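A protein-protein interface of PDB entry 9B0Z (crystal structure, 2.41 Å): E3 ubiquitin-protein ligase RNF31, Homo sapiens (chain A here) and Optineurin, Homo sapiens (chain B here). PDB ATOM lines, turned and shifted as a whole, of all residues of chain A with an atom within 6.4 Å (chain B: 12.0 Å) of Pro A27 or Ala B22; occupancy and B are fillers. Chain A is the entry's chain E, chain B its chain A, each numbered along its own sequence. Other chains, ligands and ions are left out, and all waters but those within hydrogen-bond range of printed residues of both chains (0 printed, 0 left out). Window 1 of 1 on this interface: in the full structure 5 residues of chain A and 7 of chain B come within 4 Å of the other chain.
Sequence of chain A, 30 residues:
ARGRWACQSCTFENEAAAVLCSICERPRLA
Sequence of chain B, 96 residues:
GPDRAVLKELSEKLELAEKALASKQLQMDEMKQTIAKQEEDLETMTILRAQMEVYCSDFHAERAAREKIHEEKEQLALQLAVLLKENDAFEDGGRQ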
ATOM      1  N   TRP A   5      -4.605 -11.369  22.407  1.00  0.00           N
ATOM      2  CA  TRP A   5      -4.397 -12.479  23.325  1.00  0.00           C
ATOM      3  C   TRP A   5      -3.861 -13.704  22.592  1.00  0.00           C
ATOM      4  O   TRP A   5      -4.125 -13.905  21.402  1.00  0.00           O
ATOM      5  CB  TRP A   5      -5.686 -12.835  24.073  1.00  0.00           C
ATOM      6  CG  TRP A   5      -6.821 -13.279  23.215  1.00  0.00           C
ATOM      7  CD1 TRP A   5      -7.750 -12.480  22.598  1.00  0.00           C
ATOM      8  CD2 TRP A   5      -7.197 -14.627  22.926  1.00  0.00           C
ATOM      9  NE1 TRP A   5      -8.663 -13.255  21.922  1.00  0.00           N
ATOM     10  CE2 TRP A   5      -8.347 -14.576  22.108  1.00  0.00           C
ATOM     11  CE3 TRP A   5      -6.665 -15.874  23.265  1.00  0.00           C
ATOM     12  CZ2 TRP A   5      -8.969 -15.725  21.628  1.00  0.00           C
ATOM     13  CZ3 TRP A   5      -7.288 -17.012  22.787  1.00  0.00           C
ATOM     14  CH2 TRP A   5      -8.428 -16.929  21.977  1.00  0.00           C
ATOM     15  N   CYS A   7      -3.552 -17.880  22.477  1.00  0.00           N
ATOM     16  CA  CYS A   7      -4.307 -19.044  22.908  1.00  0.00           C
ATOM     17  C   CYS A   7      -3.490 -19.879  23.881  1.00  0.00           C
ATOM     18  O   CYS A   7      -2.299 -20.114  23.670  1.00  0.00           O
ATOM     19  CB  CYS A   7      -4.701 -19.884  21.700  1.00  0.00           C
ATOM     20  SG  CYS A   7      -5.443 -21.411  22.192  1.00  0.00           S
ATOM     21  N   GLN A   8      -4.138 -20.342  24.946  1.00  0.00           N
ATOM     22  CA  GLN A   8      -3.425 -21.126  25.949  1.00  0.00           C
ATOM     23  C   GLN A   8      -3.209 -22.573  25.542  1.00  0.00           C
ATOM     24  O   GLN A   8      -2.591 -23.328  26.301  1.00  0.00           O
ATOM     25  CB  GLN A   8      -4.178 -21.071  27.279  1.00  0.00           C
ATOM     26  CG  GLN A   8      -4.077 -19.728  27.951  1.00  0.00           C
ATOM     27  CD  GLN A   8      -2.634 -19.337  28.198  1.00  0.00           C
ATOM     28  OE1 GLN A   8      -2.116 -18.406  27.578  1.00  0.00           O
ATOM     29  NE2 GLN A   8      -1.969 -20.056  29.096  1.00  0.00           N
ATOM     30  N   VAL A  19     -13.129 -14.188  20.404  1.00  0.00           N
ATOM     31  CA  VAL A  19     -13.500 -14.817  21.661  1.00  0.00           C
ATOM     32  C   VAL A  19     -13.046 -16.269  21.705  1.00  0.00           C
ATOM     33  O   VAL A  19     -12.567 -16.742  22.738  1.00  0.00           O
ATOM     34  CB  VAL A  19     -15.019 -14.710  21.920  1.00  0.00           C
ATOM     35  CG1 VAL A  19     -15.360 -13.349  22.480  1.00  0.00           C
ATOM     36  CG2 VAL A  19     -15.793 -14.961  20.644  1.00  0.00           C
ATOM     37  N   LEU A  20     -13.200 -16.988  20.597  1.00  0.00           N
ATOM     38  CA  LEU A  20     -12.613 -18.305  20.401  1.00  0.00           C
ATOM     39  C   LEU A  20     -11.304 -18.207  19.620  1.00  0.00           C
ATOM     40  O   LEU A  20     -11.116 -17.305  18.799  1.00  0.00           O
ATOM     41  CB  LEU A  20     -13.585 -19.214  19.652  1.00  0.00           C
ATOM     42  CG  LEU A  20     -14.971 -19.398  20.268  1.00  0.00           C
ATOM     43  CD1 LEU A  20     -15.817 -20.290  19.364  1.00  0.00           C
ATOM     44  CD2 LEU A  20     -14.855 -19.974  21.676  1.00  0.00           C
ATOM     45  N   CYS A  21     -10.406 -19.167  19.857  1.00  0.00           N
ATOM     46  CA  CYS A  21      -9.152 -19.196  19.106  1.00  0.00           C
ATOM     47  C   CYS A  21      -9.391 -19.357  17.611  1.00  0.00           C
ATOM     48  O   CYS A  21     -10.184 -20.197  17.179  1.00  0.00           O
ATOM     49  CB  CYS A  21      -8.261 -20.335  19.585  1.00  0.00           C
ATOM     50  SG  CYS A  21      -6.693 -20.346  18.685  1.00  0.00           S
ATOM     51  N   GLU A  25     -10.232 -22.973  18.009  1.00  0.00           N
ATOM     52  CA  GLU A  25     -11.589 -22.555  18.365  1.00  0.00           C
ATOM     53  C   GLU A  25     -11.931 -22.908  19.816  1.00  0.00           C
ATOM     54  O   GLU A  25     -13.054 -23.303  20.139  1.00  0.00           O
ATOM     55  CB  GLU A  25     -12.609 -23.132  17.379  1.00  0.00           C
ATOM     56  CG  GLU A  25     -12.131 -23.058  15.920  1.00  0.00           C
ATOM     57  CD  GLU A  25     -13.235 -23.290  14.901  1.00  0.00           C
ATOM     58  OE1 GLU A  25     -12.911 -23.506  13.711  1.00  0.00           O
ATOM     59  OE2 GLU A  25     -14.420 -23.295  15.289  1.00  0.00           O
ATOM     60  N   ARG A  26     -10.941 -22.735  20.715  1.00  0.00           N
ATOM     61  CA  ARG A  26     -11.167 -22.834  22.143  1.00  0.00           C
ATOM     62  C   ARG A  26     -11.294 -21.438  22.746  1.00  0.00           C
ATOM     63  O   ARG A  26     -10.657 -20.490  22.271  1.00  0.00           O
ATOM     64  CB  ARG A  26     -10.016 -23.570  22.826  1.00  0.00           C
ATOM     65  CG  ARG A  26      -9.714 -24.917  22.233  1.00  0.00           C
ATOM     66  CD  ARG A  26      -8.615 -25.588  23.020  1.00  0.00           C
ATOM     67  NE  ARG A  26      -8.932 -25.637  24.444  1.00  0.00           N
ATOM     68  CZ  ARG A  26      -9.541 -26.656  25.038  1.00  0.00           C
ATOM     69  NH1 ARG A  26      -9.917 -27.728  24.359  1.00  0.00           N
ATOM     70  NH2 ARG A  26      -9.766 -26.605  26.347  1.00  0.00           N
ATOM     71  N   PRO A  27     -12.113 -21.289  23.790  1.00  0.00           N
ATOM     72  CA  PRO A  27     -12.251 -19.985  24.447  1.00  0.00           C
ATOM     73  C   PRO A  27     -10.930 -19.493  25.012  1.00  0.00           C
ATOM     74  O   PRO A  27     -10.056 -20.281  25.381  1.00  0.00           O
ATOM     75  CB  PRO A  27     -13.265 -20.255  25.561  1.00  0.00           C
ATOM     76  CG  PRO A  27     -14.026 -21.431  25.093  1.00  0.00           C
ATOM     77  CD  PRO A  27     -13.040 -22.282  24.353  1.00  0.00           C
ATOM     78  N   ARG A  28     -10.795 -18.166  25.072  1.00  0.00           N
ATOM     79  CA  ARG A  28      -9.551 -17.563  25.539  1.00  0.00           C
ATOM     80  C   ARG A  28      -9.184 -18.031  26.943  1.00  0.00           C
ATOM     81  O   ARG A  28      -8.009 -18.297  27.224  1.00  0.00           O
ATOM     82  CB  ARG A  28      -9.647 -16.037  25.491  1.00  0.00           C
ATOM     83  CG  ARG A  28      -8.512 -15.348  26.241  1.00  0.00           C
ATOM     84  CD  ARG A  28      -8.643 -13.834  26.261  1.00  0.00           C
ATOM     85  NE  ARG A  28      -9.203 -13.350  27.517  1.00  0.00           N
ATOM     86  CZ  ARG A  28     -10.457 -12.949  27.655  1.00  0.00           C
ATOM     87  NH1 ARG A  28     -11.298 -12.957  26.634  1.00  0.00           N
ATOM     88  NH2 ARG A  28     -10.877 -12.524  28.844  1.00  0.00           N
ATOM     89  N   LEU A  29     -10.169 -18.164  27.834  1.00  0.00           N
ATOM     90  CA  LEU A  29      -9.905 -18.554  29.215  1.00  0.00           C
ATOM     91  C   LEU A  29      -9.903 -20.065  29.428  1.00  0.00           C
ATOM     92  O   LEU A  29     -10.129 -20.518  30.554  1.00  0.00           O
ATOM     93  CB  LEU A  29     -10.918 -17.903  30.162  1.00  0.00           C
ATOM     94  CG  LEU A  29     -10.802 -16.401  30.400  1.00  0.00           C
ATOM     95  CD1 LEU A  29     -12.036 -15.900  31.113  1.00  0.00           C
ATOM     96  CD2 LEU A  29      -9.561 -16.087  31.223  1.00  0.00           C
ATOM     97  N   ALA A  30      -9.654 -20.849  28.386  1.00  0.00           N
ATOM     98  CA  ALA A  30      -9.552 -22.295  28.555  1.00  0.00           C
ATOM     99  C   ALA A  30      -8.236 -22.840  27.999  1.00  0.00           C
ATOM    100  O   ALA A  30      -7.701 -23.826  28.512  1.00  0.00           O
ATOM    101  CB  ALA A  30     -10.733 -22.984  27.894  1.00  0.00           C
ATOM    102  OXT ALA A  30      -7.669 -22.311  27.038  1.00  0.00           O
ATOM    103  N   LYS B  13     -20.632  -8.399  31.819  1.00  0.00           N
ATOM    104  CA  LYS B  13     -21.329  -9.488  31.139  1.00  0.00           C
ATOM    105  C   LYS B  13     -20.392 -10.224  30.185  1.00  0.00           C
ATOM    106  O   LYS B  13     -20.409 -11.459  30.121  1.00  0.00           O
ATOM    107  CB  LYS B  13     -22.545  -8.950  30.393  1.00  0.00           C
ATOM    108  CG  LYS B  13     -23.762  -9.841  30.510  1.00  0.00           C
ATOM    109  CD  LYS B  13     -24.694  -9.690  29.319  1.00  0.00           C
ATOM    110  CE  LYS B  13     -26.012 -10.396  29.604  1.00  0.00           C
ATOM    111  NZ  LYS B  13     -27.129  -9.929  28.738  1.00  0.00           N
ATOM    112  N   LEU B  14     -19.570  -9.479  29.435  1.00  0.00           N
ATOM    113  CA  LEU B  14     -18.571 -10.111  28.577  1.00  0.00           C
ATOM    114  C   LEU B  14     -17.679 -11.042  29.376  1.00  0.00           C
ATOM    115  O   LEU B  14     -17.410 -12.171  28.953  1.00  0.00           O
ATOM    116  CB  LEU B  14     -17.707  -9.045  27.902  1.00  0.00           C
ATOM    117  CG  LEU B  14     -16.998  -9.375  26.584  1.00  0.00           C
ATOM    118  CD1 LEU B  14     -17.965  -9.620  25.437  1.00  0.00           C
ATOM    119  CD2 LEU B  14     -16.013  -8.257  26.257  1.00  0.00           C
ATOM    120  N   GLU B  15     -17.235 -10.597  30.553  1.00  0.00           N
ATOM    121  CA  GLU B  15     -16.398 -11.452  31.381  1.00  0.00           C
ATOM    122  C   GLU B  15     -17.171 -12.673  31.851  1.00  0.00           C
ATOM    123  O   GLU B  15     -16.619 -13.775  31.912  1.00  0.00           O
ATOM    124  CB  GLU B  15     -15.839 -10.669  32.568  1.00  0.00           C
ATOM    125  CG  GLU B  15     -14.697 -11.387  33.308  1.00  0.00           C
ATOM    126  CD  GLU B  15     -13.448 -11.593  32.443  1.00  0.00           C
ATOM    127  OE1 GLU B  15     -13.406 -11.062  31.310  1.00  0.00           O
ATOM    128  OE2 GLU B  15     -12.502 -12.280  32.894  1.00  0.00           O
ATOM    129  N   LEU B  16     -18.451 -12.502  32.186  1.00  0.00           N
ATOM    130  CA  LEU B  16     -19.245 -13.661  32.574  1.00  0.00           C
ATOM    131  C   LEU B  16     -19.425 -14.611  31.397  1.00  0.00           C
ATOM    132  O   LEU B  16     -19.327 -15.833  31.557  1.00  0.00           O
ATOM    133  CB  LEU B  16     -20.602 -13.221  33.125  1.00  0.00           C
ATOM    134  N   ALA B  17     -19.664 -14.067  30.202  1.00  0.00           N
ATOM    135  CA  ALA B  17     -19.869 -14.923  29.038  1.00  0.00           C
ATOM    136  C   ALA B  17     -18.600 -15.686  28.683  1.00  0.00           C
ATOM    137  O   ALA B  17     -18.650 -16.881  28.367  1.00  0.00           O
ATOM    138  CB  ALA B  17     -20.348 -14.086  27.852  1.00  0.00           C
ATOM    139  N   GLU B  18     -17.453 -15.016  28.725  1.00  0.00           N
ATOM    140  CA  GLU B  18     -16.199 -15.691  28.417  1.00  0.00           C
ATOM    141  C   GLU B  18     -15.818 -16.706  29.489  1.00  0.00           C
ATOM    142  O   GLU B  18     -15.190 -17.726  29.181  1.00  0.00           O
ATOM    143  CB  GLU B  18     -15.116 -14.653  28.191  1.00  0.00           C
ATOM    144  CG  GLU B  18     -15.386 -13.840  26.941  1.00  0.00           C
ATOM    145  CD  GLU B  18     -14.236 -12.946  26.597  1.00  0.00           C
ATOM    146  OE1 GLU B  18     -13.396 -12.726  27.493  1.00  0.00           O
ATOM    147  OE2 GLU B  18     -14.154 -12.479  25.442  1.00  0.00           O
ATOM    148  N   LYS B  19     -16.160 -16.436  30.751  1.00  0.00           N
ATOM    149  CA  LYS B  19     -15.959 -17.440  31.790  1.00  0.00           C
ATOM    150  C   LYS B  19     -16.841 -18.662  31.548  1.00  0.00           C
ATOM    151  O   LYS B  19     -16.391 -19.804  31.710  1.00  0.00           O
ATOM    152  CB  LYS B  19     -16.221 -16.835  33.168  1.00  0.00           C
ATOM    153  CG  LYS B  19     -15.122 -15.876  33.628  1.00  0.00           C
ATOM    154  CD  LYS B  19     -15.036 -15.789  35.142  1.00  0.00           C
ATOM    155  CE  LYS B  19     -13.668 -15.283  35.585  1.00  0.00           C
ATOM    156  NZ  LYS B  19     -13.442 -15.492  37.044  1.00  0.00           N
ATOM    157  N   ALA B  20     -18.102 -18.442  31.161  1.00  0.00           N
ATOM    158  CA  ALA B  20     -18.981 -19.564  30.839  1.00  0.00           C
ATOM    159  C   ALA B  20     -18.456 -20.350  29.642  1.00  0.00           C
ATOM    160  O   ALA B  20     -18.468 -21.588  29.651  1.00  0.00           O
ATOM    161  CB  ALA B  20     -20.403 -19.067  30.578  1.00  0.00           C
ATOM    162  N   LEU B  21     -17.985 -19.648  28.604  1.00  0.00           N
ATOM    163  CA  LEU B  21     -17.367 -20.319  27.462  1.00  0.00           C
ATOM    164  C   LEU B  21     -16.259 -21.257  27.913  1.00  0.00           C
ATOM    165  O   LEU B  21     -16.193 -22.410  27.481  1.00  0.00           O
ATOM    166  CB  LEU B  21     -16.814 -19.279  26.485  1.00  0.00           C
ATOM    167  CG  LEU B  21     -17.665 -18.751  25.334  1.00  0.00           C
ATOM    168  CD1 LEU B  21     -16.854 -17.784  24.522  1.00  0.00           C
ATOM    169  CD2 LEU B  21     -18.049 -19.915  24.450  1.00  0.00           C
ATOM    170  N   ALA B  22     -15.381 -20.779  28.794  1.00  0.00           N
ATOM    171  CA  ALA B  22     -14.344 -21.644  29.347  1.00  0.00           C
ATOM    172  C   ALA B  22     -14.961 -22.818  30.093  1.00  0.00           C
ATOM    173  O   ALA B  22     -14.583 -23.977  29.880  1.00  0.00           O
ATOM    174  CB  ALA B  22     -13.427 -20.841  30.269  1.00  0.00           C
ATOM    175  N   SER B  23     -15.941 -22.535  30.952  1.00  0.00           N
ATOM    176  CA  SER B  23     -16.565 -23.587  31.746  1.00  0.00           C
ATOM    177  C   SER B  23     -17.206 -24.642  30.856  1.00  0.00           C
ATOM    178  O   SER B  23     -17.013 -25.847  31.060  1.00  0.00           O
ATOM    179  CB  SER B  23     -17.609 -22.984  32.683  1.00  0.00           C
ATOM    180  OG  SER B  23     -18.464 -23.996  33.180  1.00  0.00           O
ATOM    181  N   LYS B  24     -17.975 -24.203  29.858  1.00  0.00           N
ATOM    182  CA  LYS B  24     -18.620 -25.159  28.974  1.00  0.00           C
ATOM    183  C   LYS B  24     -17.596 -25.950  28.178  1.00  0.00           C
ATOM    184  O   LYS B  24     -17.772 -27.156  27.980  1.00  0.00           O
ATOM    185  CB  LYS B  24     -19.594 -24.435  28.041  1.00  0.00           C
ATOM    186  CG  LYS B  24     -20.743 -23.791  28.789  1.00  0.00           C
ATOM    187  CD  LYS B  24     -22.004 -24.615  28.628  1.00  0.00           C
ATOM    188  CE  LYS B  24     -22.975 -24.345  29.762  1.00  0.00           C
ATOM    189  NZ  LYS B  24     -24.163 -25.247  29.694  1.00  0.00           N
ATOM    190  N   GLN B  25     -16.491 -25.319  27.779  1.00  0.00           N
ATOM    191  CA  GLN B  25     -15.480 -26.052  27.024  1.00  0.00           C
ATOM    192  C   GLN B  25     -14.787 -27.084  27.897  1.00  0.00           C
ATOM    193  O   GLN B  25     -14.485 -28.192  27.438  1.00  0.00           O
ATOM    194  CB  GLN B  25     -14.458 -25.091  26.428  1.00  0.00           C
ATOM    195  CG  GLN B  25     -13.295 -25.797  25.763  1.00  0.00           C
ATOM    196  CD  GLN B  25     -13.624 -26.306  24.375  1.00  0.00           C
ATOM    197  OE1 GLN B  25     -14.082 -25.552  23.519  1.00  0.00           O
ATOM    198  NE2 GLN B  25     -13.389 -27.587  24.147  1.00  0.00           N
ATOM    199  N   LEU B  26     -14.548 -26.747  29.163  1.00  0.00           N
ATOM    200  CA  LEU B  26     -14.015 -27.724  30.104  1.00  0.00           C
ATOM    201  C   LEU B  26     -14.950 -28.920  30.211  1.00  0.00           C
ATOM    202  O   LEU B  26     -14.511 -30.074  30.194  1.00  0.00           O
ATOM    203  CB  LEU B  26     -13.824 -27.066  31.469  1.00  0.00           C
ATOM    204  CG  LEU B  26     -12.695 -26.034  31.530  1.00  0.00           C
ATOM    205  CD1 LEU B  26     -12.219 -25.817  32.960  1.00  0.00           C
ATOM    206  CD2 LEU B  26     -11.545 -26.450  30.630  1.00  0.00           C
ATOM    207  N   GLN B  27     -16.255 -28.654  30.324  1.00  0.00           N
ATOM    208  CA  GLN B  27     -17.239 -29.728  30.341  1.00  0.00           C
ATOM    209  C   GLN B  27     -17.085 -30.614  29.112  1.00  0.00           C
ATOM    210  O   GLN B  27     -17.024 -31.844  29.222  1.00  0.00           O
ATOM    211  CB  GLN B  27     -18.648 -29.137  30.405  1.00  0.00           C
ATOM    212  CG  GLN B  27     -18.985 -28.545  31.761  1.00  0.00           C
ATOM    213  CD  GLN B  27     -20.390 -27.973  31.840  1.00  0.00           C
ATOM    214  OE1 GLN B  27     -21.250 -28.262  31.006  1.00  0.00           O
ATOM    215  NE2 GLN B  27     -20.607 -27.104  32.817  1.00  0.00           N
ATOM    216  N   MET B  28     -16.969 -29.996  27.932  1.00  0.00           N
ATOM    217  CA  MET B  28     -16.796 -30.769  26.709  1.00  0.00           C
ATOM    218  C   MET B  28     -15.535 -31.612  26.766  1.00  0.00           C
ATOM    219  O   MET B  28     -15.528 -32.761  26.304  1.00  0.00           O
ATOM    220  CB  MET B  28     -16.743 -29.838  25.498  1.00  0.00           C
ATOM    221  CG  MET B  28     -18.039 -29.142  25.194  1.00  0.00           C
ATOM    222  SD  MET B  28     -17.787 -27.841  23.998  1.00  0.00           S
ATOM    223  CE  MET B  28     -17.628 -28.810  22.510  1.00  0.00           C
ATOM    224  N   ASP B  29     -14.463 -31.061  27.339  1.00  0.00           N
ATOM    225  CA  ASP B  29     -13.217 -31.813  27.445  1.00  0.00           C
ATOM    226  C   ASP B  29     -13.413 -33.076  28.268  1.00  0.00           C
ATOM    227  O   ASP B  29     -12.912 -34.144  27.902  1.00  0.00           O
ATOM    228  CB  ASP B  29     -12.126 -30.922  28.051  1.00  0.00           C
ATOM    229  CG  ASP B  29     -11.741 -29.753  27.137  1.00  0.00           C
ATOM    230  OD1 ASP B  29     -10.813 -28.991  27.487  1.00  0.00           O
ATOM    231  OD2 ASP B  29     -12.400 -29.559  26.093  1.00  0.00           O
ATOM    232  N   GLU B  30     -14.170 -32.983  29.366  1.00  0.00           N
ATOM    233  CA  GLU B  30     -14.442 -34.163  30.183  1.00  0.00           C
ATOM    234  C   GLU B  30     -15.238 -35.202  29.404  1.00  0.00           C
ATOM    235  O   GLU B  30     -14.907 -36.393  29.427  1.00  0.00           O
ATOM    236  CB  GLU B  30     -15.196 -33.764  31.454  1.00  0.00           C
ATOM    237  N   MET B  31     -16.272 -34.769  28.675  1.00  0.00           N
ATOM    238  CA  MET B  31     -17.096 -35.735  27.959  1.00  0.00           C
ATOM    239  C   MET B  31     -16.361 -36.326  26.769  1.00  0.00           C
ATOM    240  O   MET B  31     -16.581 -37.491  26.422  1.00  0.00           O
ATOM    241  CB  MET B  31     -18.392 -35.102  27.473  1.00  0.00           C
ATOM    242  CG  MET B  31     -18.854 -33.928  28.272  1.00  0.00           C
ATOM    243  SD  MET B  31     -20.460 -33.354  27.716  1.00  0.00           S
ATOM    244  CE  MET B  31     -21.513 -34.635  28.398  1.00  0.00           C
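CG1 of Val A19 touches OE2 of Glu B18 (3.3 Å).
O of Leu B21 touches CG of Pro A27, at 3.4 Å.
Ala B22 touches Pro A27.
CD of Pro A27 touches OE1 of Gln B25, at 3.5 Å.
Leu A29 touches Lys B19 (CD1 to CG, 3.98 Å).
Leu A29 touches Ala B22.
No residue of chain B comes within 4 Å of Cys A7.
Of chain B, only Glu B18 (3.3 Å) comes within 4 Å of Val A19.
Leu A20 touches none of the printed residues of chain B.
Of chain B, only Leu B21 (3.4 Å), Ala B22 (3.9 Å) and Gln B25 (3.5 Å) come within 4 Å of Pro A27.
Lys B13 touches none of the printed residues of chain A.
Of the printed residues of chain A, Glu B15 touches Arg A28 (3.8 Å).
Ala B17 touches none of the printed residues of chain A.
Printed residues of chain A within 4 Å of Glu B18: Val A19 (3.3 Å) and Arg A28 (2.3 Å).
Of the printed residues of chain A, Leu B21 touches Pro A27.
Of chain A, only Pro A27 and Leu A29 come within 4 Å of Ala B22.
Of the printed residues of chain A, Asp B29 touches Arg A26 (2.8 Å).
The nearest residue of chain A that does not touch Ala B22 is Ala A30 (4.1 Å).
The nearest printed residue of chain A that does not touch Asp B29 is Ala A30 (6.0 Å).
The side-chain carboxylate (OD2) of Asp B29 is in hydrogen-bond range of the side-chain amide nitrogen (NE2) of Gln B25, 2.9 Å away.
N of Cys A21 lies within hydrogen-bond range of O of Arg A26, 2.8 Å away.
The backbone carbonyl oxygen of Val A19 is in hydrogen-bond range of the backbone NH of Arg A28.
Of the 12 printed residues of chain A, 5 touch a printed residue of chain B.
Hydrophobic or aromatic side chains of chain A within 4 Å of the printed part of chain B: Val A19, Pro A27 and Leu A29.
Of the 19 printed residues of chain B, 7 touch a printed residue of chain A.
Hydrophobic or aromatic side chains of chain B within 4 Å of the printed part of chain A: Leu B21 and Ala B22.
Among the printed residues, 10 pairs touch across the chains.
Among the printed residues, Asp or Glu carboxylates within 4 Å of a Lys or Arg side-chain nitrogen of the other chain: Arg A26 with Asp B29, Arg A28 with Glu B15 and Arg A28 with Glu B18.
The side-chain carboxylate of Glu B18 is in salt-bridge range of the guanidinium group of Arg A28, 2.9 Å away.
The side-chain amide nitrogen (NE2) of Gln B25 sits close to the guanidinium group (NH1) of Arg A26, 3.5 Å away.
The side-chain carboxylate (OD1) of Asp B29 is in salt-bridge range of the guanidinium group (NH2) of Arg A26, at 2.8 Å.
NH2 of Arg A28 is in salt-bridge range of OE1 of Glu B15, at 3.8 Å.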
